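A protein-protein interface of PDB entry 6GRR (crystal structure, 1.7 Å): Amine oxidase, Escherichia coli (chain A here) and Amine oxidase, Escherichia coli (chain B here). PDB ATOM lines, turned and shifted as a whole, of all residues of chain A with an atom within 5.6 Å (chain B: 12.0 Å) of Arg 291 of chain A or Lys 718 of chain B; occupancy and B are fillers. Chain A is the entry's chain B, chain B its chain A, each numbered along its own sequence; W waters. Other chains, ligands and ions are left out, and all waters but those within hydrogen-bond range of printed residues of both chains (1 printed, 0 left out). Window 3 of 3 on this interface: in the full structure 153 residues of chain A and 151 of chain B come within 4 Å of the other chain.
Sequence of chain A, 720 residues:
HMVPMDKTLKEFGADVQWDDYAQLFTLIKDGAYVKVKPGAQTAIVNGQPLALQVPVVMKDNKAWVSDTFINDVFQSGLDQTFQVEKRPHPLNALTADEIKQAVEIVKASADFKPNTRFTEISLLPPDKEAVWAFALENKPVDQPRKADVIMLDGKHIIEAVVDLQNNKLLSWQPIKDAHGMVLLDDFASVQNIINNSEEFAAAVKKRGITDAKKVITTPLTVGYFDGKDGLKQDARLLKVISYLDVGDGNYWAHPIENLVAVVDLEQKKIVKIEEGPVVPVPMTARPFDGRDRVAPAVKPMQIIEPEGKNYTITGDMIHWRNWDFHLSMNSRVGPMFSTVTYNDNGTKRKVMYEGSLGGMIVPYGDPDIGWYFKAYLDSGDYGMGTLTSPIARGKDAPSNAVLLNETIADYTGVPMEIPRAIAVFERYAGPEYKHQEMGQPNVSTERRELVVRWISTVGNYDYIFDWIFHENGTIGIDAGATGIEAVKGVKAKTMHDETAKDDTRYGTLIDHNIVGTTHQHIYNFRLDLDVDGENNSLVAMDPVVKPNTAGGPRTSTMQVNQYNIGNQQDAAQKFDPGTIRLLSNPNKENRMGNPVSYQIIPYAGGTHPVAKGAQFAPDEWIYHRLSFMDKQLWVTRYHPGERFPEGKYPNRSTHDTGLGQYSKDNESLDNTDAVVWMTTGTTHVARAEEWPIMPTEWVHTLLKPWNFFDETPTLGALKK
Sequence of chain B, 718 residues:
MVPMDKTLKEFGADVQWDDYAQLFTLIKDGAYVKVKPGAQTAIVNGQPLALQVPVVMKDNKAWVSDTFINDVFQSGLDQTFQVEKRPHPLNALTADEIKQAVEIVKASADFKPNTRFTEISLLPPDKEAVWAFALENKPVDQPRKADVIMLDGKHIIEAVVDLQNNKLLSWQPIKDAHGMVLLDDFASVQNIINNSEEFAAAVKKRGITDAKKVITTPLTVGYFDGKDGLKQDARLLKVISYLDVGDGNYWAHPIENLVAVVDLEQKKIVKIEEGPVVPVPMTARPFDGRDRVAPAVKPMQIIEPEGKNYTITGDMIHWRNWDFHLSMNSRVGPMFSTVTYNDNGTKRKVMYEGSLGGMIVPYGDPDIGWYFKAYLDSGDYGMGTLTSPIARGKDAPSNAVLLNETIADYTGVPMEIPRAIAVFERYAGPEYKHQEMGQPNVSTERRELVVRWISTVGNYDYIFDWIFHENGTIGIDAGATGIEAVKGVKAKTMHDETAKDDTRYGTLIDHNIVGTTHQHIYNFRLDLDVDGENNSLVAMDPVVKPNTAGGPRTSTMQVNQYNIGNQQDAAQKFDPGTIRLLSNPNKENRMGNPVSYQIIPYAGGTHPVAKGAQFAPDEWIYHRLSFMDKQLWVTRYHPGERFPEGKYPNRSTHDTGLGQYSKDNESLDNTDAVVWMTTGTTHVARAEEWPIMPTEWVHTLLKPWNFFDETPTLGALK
Water W1 bridges the backbone carbonyl oxygen (O) of Asp 292 of chain A (2.9 Å) and the backbone NH (N) of Lys 718 of chain B (3.2 Å).
Of the 18 printed residues of chain B, 7 touch a printed residue of chain A. Printed residues of chain B that touch a printed residue of chain A: Val 442, Glu 710, Leu 714, Gly 715, Ala 716, Leu 717 and Lys 718. Hydrophobic or aromatic side chains of chain B that line the printed part of chain A: Val 442, Leu 714 and Leu 717. Of the 10 printed residues of chain A, 5 touch a printed residue of chain B. Printed residues of chain A that touch a printed residue of chain B: Asp 289, Arg 291, Asp 292, Arg 293 and Val 294. Among the printed residues, 13 pairs touch across the chains. Among the printed residues, Asp or Glu carboxylates within 4 Å of a Lys or Arg side-chain nitrogen of the other chain: Arg 293 of chain A with Glu 710 of chain B (2.8 Å).
Gly 247 of chain A touches none of the printed residues of chain B. No residue of chain B comes within 4 Å of Gly 249 of chain A. No residue of chain B comes within 4 Å of Pro 287 of chain A. Of the printed residues of chain B, Asp 289 of chain A touches Val 442 (3.5 Å). No residue of chain B comes within 4 Å of Gly 290 of chain A. Of chain B, only Lys 718 (2.9 Å) comes within 4 Å of Arg 291 of chain A. Asp 292 of chain A touches two residues of chain B. Of the printed residues of chain A, Val 442 of chain B touches Asp 289 (3.5 Å). Ser 443 of chain B touches none of the printed residues of chain A. Thr 444 of chain B touches none of the printed residues of chain A. Of the printed residues of chain A, Leu 717 of chain B touches Asp 292, Arg 293 and Val 294. The nearest residue of chain A that does not touch Lys 718 of chain B is Gly 290 of chain A (4.4 Å).
Asp 289 of chain A touches Val 442 of chain B (CB to CG2, 3.5 Å). Leu 717 of chain B touches Asp 292 of chain A (CA to O, 3.5 Å). Arg 293 of chain A touches Leu 714 of chain B. Arg 293 of chain A touches Ala 716 of chain B. CD2 of Leu 717 of chain B touches CZ of Arg 293 of chain A, at 3.7 Å. Lys 718 of chain B touches Arg 293 of chain A (NZ to O, 3.6 Å). Val 294 of chain A touches Leu 717 of chain B (CG2 to O, 3.98 Å). CG of Lys 718 of chain B touches N of Val 294 of chain A (3.9 Å).
The backbone NH (N) of His 434 of chain B sits at hydrogen-bond distance from the backbone carbonyl oxygen (O) of Val 442 of chain B (2.9 Å). NH1 of Arg 291 of chain A lies within hydrogen-bond range of O of Gly 247 of chain A. The guanidinium group of Arg 291 of chain A sits close to the backbone carbonyl oxygen of Asp 248 of chain A. The side-chain carboxylate (OD1) of Asp 289 of chain A lies within salt-bridge range of the guanidinium group (NE) of Arg 291 of chain A (2.9 Å). The side-chain carboxylate (OD1) of Asp 292 of chain A is in salt-bridge range of the guanidinium group (NE) of Arg 293 of chain A, at 3.3 Å.
The side-chain carboxylate of Glu 710 of chain B is in salt-bridge range of the guanidinium group of Arg 293 of chain A (2.8 Å). O of Gly 715 of chain B lies within hydrogen-bond range of NH1 of Arg 293 of chain A. The backbone carbonyl oxygen (O) of Ala 716 of chain B sits at hydrogen-bond distance from the backbone NH (N) of Val 294 of chain A, 2.9 Å away. O of Arg 291 of chain A sits at hydrogen-bond distance from NZ of Lys 718 of chain B (2.9 Å). The backbone carbonyl oxygen (O) of Asp 292 of chain A lies within hydrogen-bond range of the backbone NH (N) of Lys 718 of chain B.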
ATOM      1  N   GLY A 247       7.334  28.500  26.881  1.00  0.00           N
ATOM      2  CA  GLY A 247       7.590  27.218  27.548  1.00  0.00           C
ATOM      3  C   GLY A 247       8.617  26.334  26.868  1.00  0.00           C
ATOM      4  O   GLY A 247       8.675  25.146  27.129  1.00  0.00           O
ATOM      5  N   ASP A 248       9.465  26.916  26.020  1.00  0.00           N
ATOM      6  CA  ASP A 248      10.509  26.151  25.329  1.00  0.00           C
ATOM      7  C   ASP A 248      11.888  26.342  25.968  1.00  0.00           C
ATOM      8  O   ASP A 248      12.871  25.804  25.462  1.00  0.00           O
ATOM      9  CB  ASP A 248      10.544  26.512  23.824  1.00  0.00           C
ATOM     10  CG  ASP A 248      10.897  27.977  23.556  1.00  0.00           C
ATOM     11  OD1 ASP A 248      11.065  28.782  24.496  1.00  0.00           O
ATOM     12  OD2 ASP A 248      11.009  28.336  22.357  1.00  0.00           O
ATOM     13  N   GLY A 249      11.953  27.102  27.057  1.00  0.00           N
ATOM     14  CA  GLY A 249      13.220  27.419  27.739  1.00  0.00           C
ATOM     15  C   GLY A 249      14.053  28.481  27.060  1.00  0.00           C
ATOM     16  O   GLY A 249      15.144  28.817  27.537  1.00  0.00           O
ATOM     17  N   PRO A 287      13.706  25.245  21.469  1.00  0.00           N
ATOM     18  CA  PRO A 287      14.563  24.874  22.612  1.00  0.00           C
ATOM     19  C   PRO A 287      16.015  24.599  22.186  1.00  0.00           C
ATOM     20  O   PRO A 287      16.260  24.075  21.099  1.00  0.00           O
ATOM     21  CB  PRO A 287      13.937  23.590  23.129  1.00  0.00           C
ATOM     22  CG  PRO A 287      13.186  23.020  21.988  1.00  0.00           C
ATOM     23  CD  PRO A 287      12.724  24.192  21.161  1.00  0.00           C
ATOM     24  N   ASP A 289      18.048  23.075  24.694  1.00  0.00           N
ATOM     25  CA  ASP A 289      18.533  22.200  25.784  1.00  0.00           C
ATOM     26  C   ASP A 289      18.456  20.715  25.488  1.00  0.00           C
ATOM     27  O   ASP A 289      18.773  19.887  26.359  1.00  0.00           O
ATOM     28  CB  ASP A 289      17.866  22.540  27.130  1.00  0.00           C
ATOM     29  CG  ASP A 289      16.395  22.129  27.208  1.00  0.00           C
ATOM     30  OD1 ASP A 289      15.805  21.735  26.170  1.00  0.00           O
ATOM     31  OD2 ASP A 289      15.822  22.240  28.328  1.00  0.00           O
ATOM     32  N   GLY A 290      18.050  20.372  24.267  1.00  0.00           N
ATOM     33  CA  GLY A 290      17.955  19.005  23.844  1.00  0.00           C
ATOM     34  C   GLY A 290      16.659  18.279  24.142  1.00  0.00           C
ATOM     35  O   GLY A 290      16.573  17.088  23.878  1.00  0.00           O
ATOM     36  N   ARG A 291      15.663  18.969  24.689  1.00  0.00           N
ATOM     37  CA  ARG A 291      14.410  18.303  25.088  1.00  0.00           C
ATOM     38  C   ARG A 291      13.699  17.636  23.907  1.00  0.00           C
ATOM     39  O   ARG A 291      13.043  16.616  24.092  1.00  0.00           O
ATOM     40  CB  ARG A 291      13.472  19.275  25.803  1.00  0.00           C
ATOM     41  CG  ARG A 291      12.964  20.404  24.915  1.00  0.00           C
ATOM     42  CD  ARG A 291      12.158  21.411  25.689  1.00  0.00           C
ATOM     43  NE  ARG A 291      12.967  22.218  26.594  1.00  0.00           N
ATOM     44  CZ  ARG A 291      12.476  23.111  27.443  1.00  0.00           C
ATOM     45  NH1 ARG A 291      11.158  23.349  27.513  1.00  0.00           N
ATOM     46  NH2 ARG A 291      13.299  23.782  28.230  1.00  0.00           N
ATOM     47  N   ASP A 292      13.853  18.211  22.714  1.00  0.00           N
ATOM     48  CA  ASP A 292      13.248  17.697  21.478  1.00  0.00           C
ATOM     49  C   ASP A 292      14.218  16.889  20.613  1.00  0.00           C
ATOM     50  O   ASP A 292      13.875  16.548  19.480  1.00  0.00           O
ATOM     51  CB  ASP A 292      12.641  18.856  20.641  1.00  0.00           C
ATOM     52  CG  ASP A 292      13.678  19.913  20.203  1.00  0.00           C
ATOM     53  OD1 ASP A 292      14.798  19.987  20.791  1.00  0.00           O
ATOM     54  OD2 ASP A 292      13.344  20.706  19.283  1.00  0.00           O
ATOM     55  N   ARG A 293      15.406  16.566  21.141  1.00  0.00           N
ATOM     56  CA  ARG A 293      16.472  15.917  20.355  1.00  0.00           C
ATOM     57  C   ARG A 293      16.807  14.528  20.877  1.00  0.00           C
ATOM     58  O   ARG A 293      16.665  14.258  22.063  1.00  0.00           O
ATOM     59  CB  ARG A 293      17.759  16.755  20.380  1.00  0.00           C
ATOM     60  CG  ARG A 293      17.586  18.216  19.992  1.00  0.00           C
ATOM     61  CD  ARG A 293      17.237  18.368  18.534  1.00  0.00           C
ATOM     62  NE  ARG A 293      16.790  19.722  18.185  1.00  0.00           N
ATOM     63  CZ  ARG A 293      16.940  20.302  16.992  1.00  0.00           C
ATOM     64  NH1 ARG A 293      17.569  19.687  15.988  1.00  0.00           N
ATOM     65  NH2 ARG A 293      16.476  21.539  16.812  1.00  0.00           N
ATOM     66  N   VAL A 294      17.300  13.680  19.979  1.00  0.00           N
ATOM     67  CA  VAL A 294      17.822  12.374  20.345  1.00  0.00           C
ATOM     68  C   VAL A 294      19.200  12.557  20.995  1.00  0.00           C
ATOM     69  O   VAL A 294      20.034  13.323  20.506  1.00  0.00           O
ATOM     70  CB  VAL A 294      17.939  11.470  19.115  1.00  0.00           C
ATOM     71  CG1 VAL A 294      18.643  10.163  19.465  1.00  0.00           C
ATOM     72  CG2 VAL A 294      16.560  11.190  18.536  1.00  0.00           C
ATOM     73  N   ASN B 344      21.059  14.776   8.380  1.00  0.00           N
ATOM     74  CA  ASN B 344      19.833  14.050   8.759  1.00  0.00           C
ATOM     75  C   ASN B 344      19.496  12.922   7.756  1.00  0.00           C
ATOM     76  O   ASN B 344      18.341  12.739   7.343  1.00  0.00           O
ATOM     77  CB  ASN B 344      18.688  15.081   8.944  1.00  0.00           C
ATOM     78  CG  ASN B 344      17.424  14.490   9.585  1.00  0.00           C
ATOM     79  OD1 ASN B 344      16.314  14.780   9.130  1.00  0.00           O
ATOM     80  ND2 ASN B 344      17.582  13.661  10.617  1.00  0.00           N
ATOM     81  N   TYR B 432      28.975  24.374  22.371  1.00  0.00           N
ATOM     82  CA  TYR B 432      28.233  25.564  22.712  1.00  0.00           C
ATOM     83  C   TYR B 432      27.868  25.497  24.173  1.00  0.00           C
ATOM     84  O   TYR B 432      27.962  24.436  24.810  1.00  0.00           O
ATOM     85  CB  TYR B 432      26.962  25.696  21.865  1.00  0.00           C
ATOM     86  CG  TYR B 432      26.053  24.477  21.825  1.00  0.00           C
ATOM     87  CD1 TYR B 432      25.290  24.104  22.927  1.00  0.00           C
ATOM     88  CD2 TYR B 432      25.930  23.717  20.671  1.00  0.00           C
ATOM     89  CE1 TYR B 432      24.453  22.991  22.878  1.00  0.00           C
ATOM     90  CE2 TYR B 432      25.095  22.612  20.612  1.00  0.00           C
ATOM     91  CZ  TYR B 432      24.351  22.264  21.712  1.00  0.00           C
ATOM     92  OH  TYR B 432      23.525  21.164  21.669  1.00  0.00           O
ATOM     93  N   HIS B 434      24.997  27.654  27.050  1.00  0.00           N
ATOM     94  CA  HIS B 434      24.267  28.800  27.596  1.00  0.00           C
ATOM     95  C   HIS B 434      23.845  28.527  29.003  1.00  0.00           C
ATOM     96  O   HIS B 434      23.147  27.555  29.216  1.00  0.00           O
ATOM     97  CB  HIS B 434      23.029  29.197  26.779  1.00  0.00           C
ATOM     98  CG  HIS B 434      22.377  30.439  27.301  1.00  0.00           C
ATOM     99  ND1 HIS B 434      23.084  31.597  27.522  1.00  0.00           N
ATOM    100  CD2 HIS B 434      21.104  30.691  27.692  1.00  0.00           C
ATOM    101  CE1 HIS B 434      22.272  32.520  27.999  1.00  0.00           C
ATOM    102  NE2 HIS B 434      21.061  31.998  28.107  1.00  0.00           N
ATOM    103  N   GLU B 436      21.638  30.233  31.314  1.00  0.00           N
ATOM    104  CA  GLU B 436      20.579  31.193  31.610  1.00  0.00           C
ATOM    105  C   GLU B 436      20.493  31.420  33.133  1.00  0.00           C
ATOM    106  O   GLU B 436      20.565  30.461  33.921  1.00  0.00           O
ATOM    107  CB  GLU B 436      19.238  30.700  31.029  1.00  0.00           C
ATOM    108  CG  GLU B 436      18.073  31.679  31.202  1.00  0.00           C
ATOM    109  CD  GLU B 436      18.269  33.008  30.460  1.00  0.00           C
ATOM    110  OE1 GLU B 436      18.847  33.001  29.334  1.00  0.00           O
ATOM    111  OE2 GLU B 436      17.845  34.076  30.990  1.00  0.00           O
ATOM    112  N   GLY B 438      19.619  31.623  36.747  1.00  0.00           N
ATOM    113  CA  GLY B 438      18.633  30.884  37.540  1.00  0.00           C
ATOM    114  C   GLY B 438      18.067  29.611  36.933  1.00  0.00           C
ATOM    115  O   GLY B 438      17.130  29.055  37.480  1.00  0.00           O
ATOM    116  N   GLN B 439      18.647  29.119  35.833  1.00  0.00           N
ATOM    117  CA  GLN B 439      18.171  27.921  35.161  1.00  0.00           C
ATOM    118  C   GLN B 439      19.274  26.873  35.100  1.00  0.00           C
ATOM    119  O   GLN B 439      20.430  27.184  35.390  1.00  0.00           O
ATOM    120  CB  GLN B 439      17.721  28.250  33.731  1.00  0.00           C
ATOM    121  CG  GLN B 439      16.594  29.258  33.622  1.00  0.00           C
ATOM    122  CD  GLN B 439      15.324  28.789  34.291  1.00  0.00           C
ATOM    123  OE1 GLN B 439      14.658  29.569  34.961  1.00  0.00           O
ATOM    124  NE2 GLN B 439      15.004  27.509  34.146  1.00  0.00           N
ATOM    125  N   PRO B 440      18.918  25.619  34.759  1.00  0.00           N
ATOM    126  CA  PRO B 440      19.955  24.608  34.570  1.00  0.00           C
ATOM    127  C   PRO B 440      20.824  24.944  33.354  1.00  0.00           C
ATOM    128  O   PRO B 440      20.312  25.392  32.329  1.00  0.00           O
ATOM    129  CB  PRO B 440      19.171  23.313  34.329  1.00  0.00           C
ATOM    130  CG  PRO B 440      17.804  23.574  34.872  1.00  0.00           C
ATOM    131  CD  PRO B 440      17.565  25.032  34.688  1.00  0.00           C
ATOM    132  N   ASN B 441      22.121  24.748  33.519  1.00  0.00           N
ATOM    133  CA  ASN B 441      23.089  24.918  32.431  1.00  0.00           C
ATOM    134  C   ASN B 441      22.815  24.033  31.222  1.00  0.00           C
ATOM    135  O   ASN B 441      22.290  22.919  31.353  1.00  0.00           O
ATOM    136  CB  ASN B 441      24.473  24.575  32.915  1.00  0.00           C
ATOM    137  CG  ASN B 441      25.512  24.806  31.838  1.00  0.00           C
ATOM    138  OD1 ASN B 441      25.658  25.936  31.349  1.00  0.00           O
ATOM    139  ND2 ASN B 441      26.206  23.749  31.442  1.00  0.00           N
ATOM    140  N   VAL B 442      23.194  24.531  30.046  1.00  0.00           N
ATOM    141  CA  VAL B 442      23.245  23.731  28.829  1.00  0.00           C
ATOM    142  C   VAL B 442      24.685  23.857  28.315  1.00  0.00           C
ATOM    143  O   VAL B 442      25.123  24.959  28.044  1.00  0.00           O
ATOM    144  CB  VAL B 442      22.247  24.213  27.765  1.00  0.00           C
ATOM    145  CG1 VAL B 442      22.450  23.480  26.442  1.00  0.00           C
ATOM    146  CG2 VAL B 442      20.802  24.045  28.243  1.00  0.00           C
ATOM    147  N   SER B 443      25.406  22.740  28.225  1.00  0.00           N
ATOM    148  CA  SER B 443      26.750  22.709  27.625  1.00  0.00           C
ATOM    149  C   SER B 443      26.900  21.403  26.888  1.00  0.00           C
ATOM    150  O   SER B 443      26.419  20.376  27.354  1.00  0.00           O
ATOM    151  CB  SER B 443      27.866  22.739  28.678  1.00  0.00           C
ATOM    152  OG  SER B 443      28.005  23.995  29.259  1.00  0.00           O
ATOM    153  N   THR B 444      27.594  21.423  25.754  1.00  0.00           N
ATOM    154  CA  THR B 444      28.018  20.186  25.104  1.00  0.00           C
ATOM    155  C   THR B 444      29.478  20.306  24.710  1.00  0.00           C
ATOM    156  O   THR B 444      29.953  21.404  24.432  1.00  0.00           O
ATOM    157  CB  THR B 444      27.215  19.890  23.819  1.00  0.00           C
ATOM    158  OG1 THR B 444      27.376  20.981  22.910  1.00  0.00           O
ATOM    159  CG2 THR B 444      25.734  19.736  24.118  1.00  0.00           C
ATOM    160  N   GLU B 710      19.877  25.350  10.892  1.00  0.00           N
ATOM    161  CA  GLU B 710      19.943  25.571  12.321  1.00  0.00           C
ATOM    162  C   GLU B 710      21.297  25.059  12.811  1.00  0.00           C
ATOM    163  O   GLU B 710      22.050  24.428  12.043  1.00  0.00           O
ATOM    164  CB  GLU B 710      18.821  24.823  13.069  1.00  0.00           C
ATOM    165  CG  GLU B 710      18.869  23.309  12.894  1.00  0.00           C
ATOM    166  CD  GLU B 710      17.842  22.557  13.746  1.00  0.00           C
ATOM    167  OE1 GLU B 710      16.969  23.170  14.390  1.00  0.00           O
ATOM    168  OE2 GLU B 710      17.936  21.325  13.788  1.00  0.00           O
ATOM    169  N   THR B 713      24.824  20.790  15.372  1.00  0.00           N
ATOM    170  CA  THR B 713      25.159  19.833  16.441  1.00  0.00           C
ATOM    171  C   THR B 713      24.084  19.673  17.527  1.00  0.00           C
ATOM    172  O   THR B 713      24.344  19.059  18.565  1.00  0.00           O
ATOM    173  CB  THR B 713      26.457  20.314  17.144  1.00  0.00           C
ATOM    174  OG1 THR B 713      26.406  21.728  17.293  1.00  0.00           O
ATOM    175  CG2 THR B 713      27.648  19.992  16.280  1.00  0.00           C
ATOM    176  N   LEU B 714      22.878  20.203  17.310  1.00  0.00           N
ATOM    177  CA  LEU B 714      21.774  19.992  18.263  1.00  0.00           C
ATOM    178  C   LEU B 714      21.319  18.543  18.313  1.00  0.00           C
ATOM    179  O   LEU B 714      20.912  18.064  19.369  1.00  0.00           O
ATOM    180  CB  LEU B 714      20.571  20.884  17.925  1.00  0.00           C
ATOM    181  CG  LEU B 714      20.539  22.252  18.581  1.00  0.00           C
ATOM    182  CD1 LEU B 714      19.289  22.963  18.097  1.00  0.00           C
ATOM    183  CD2 LEU B 714      20.523  22.164  20.093  1.00  0.00           C
ATOM    184  N   GLY B 715      21.395  17.862  17.174  1.00  0.00           N
ATOM    185  CA  GLY B 715      21.062  16.461  17.090  1.00  0.00           C
ATOM    186  C   GLY B 715      19.783  16.295  16.307  1.00  0.00           C
ATOM    187  O   GLY B 715      19.070  17.264  16.027  1.00  0.00           O
ATOM    188  N   ALA B 716      19.494  15.056  15.960  1.00  0.00           N
ATOM    189  CA  ALA B 716      18.272  14.726  15.224  1.00  0.00           C
ATOM    190  C   ALA B 716      17.064  14.961  16.124  1.00  0.00           C
ATOM    191  O   ALA B 716      17.156  14.845  17.353  1.00  0.00           O
ATOM    192  CB  ALA B 716      18.308  13.286  14.763  1.00  0.00           C
ATOM    193  N   LEU B 717      15.946  15.317  15.507  1.00  0.00           N
ATOM    194  CA  LEU B 717      14.683  15.463  16.229  1.00  0.00           C
ATOM    195  C   LEU B 717      14.139  14.101  16.671  1.00  0.00           C
ATOM    196  O   LEU B 717      14.244  13.122  15.944  1.00  0.00           O
ATOM    197  CB  LEU B 717      13.644  16.193  15.358  1.00  0.00           C
ATOM    198  CG  LEU B 717      13.906  17.678  15.104  1.00  0.00           C
ATOM    199  CD1 LEU B 717      12.935  18.201  14.052  1.00  0.00           C
ATOM    200  CD2 LEU B 717      13.801  18.507  16.373  1.00  0.00           C
ATOM    201  N   LYS B 718      13.614  14.032  17.891  1.00  0.00           N
ATOM    202  CA  LYS B 718      12.788  12.895  18.297  1.00  0.00           C
ATOM    203  C   LYS B 718      11.520  12.821  17.434  1.00  0.00           C
ATOM    204  O   LYS B 718      11.065  11.734  17.111  1.00  0.00           O
ATOM    205  CB  LYS B 718      12.386  13.022  19.763  1.00  0.00           C
ATOM    206  CG  LYS B 718      13.533  12.819  20.731  1.00  0.00           C
ATOM    207  CD  LYS B 718      13.057  12.293  22.079  1.00  0.00           C
ATOM    208  CE  LYS B 718      12.587  13.396  23.000  1.00  0.00           C
ATOM    209  NZ  LYS B 718      13.671  13.755  23.948  1.00  0.00           N
HETATM  210  O   HOH W   1      11.164  16.042  18.466  1.00  0.00           O
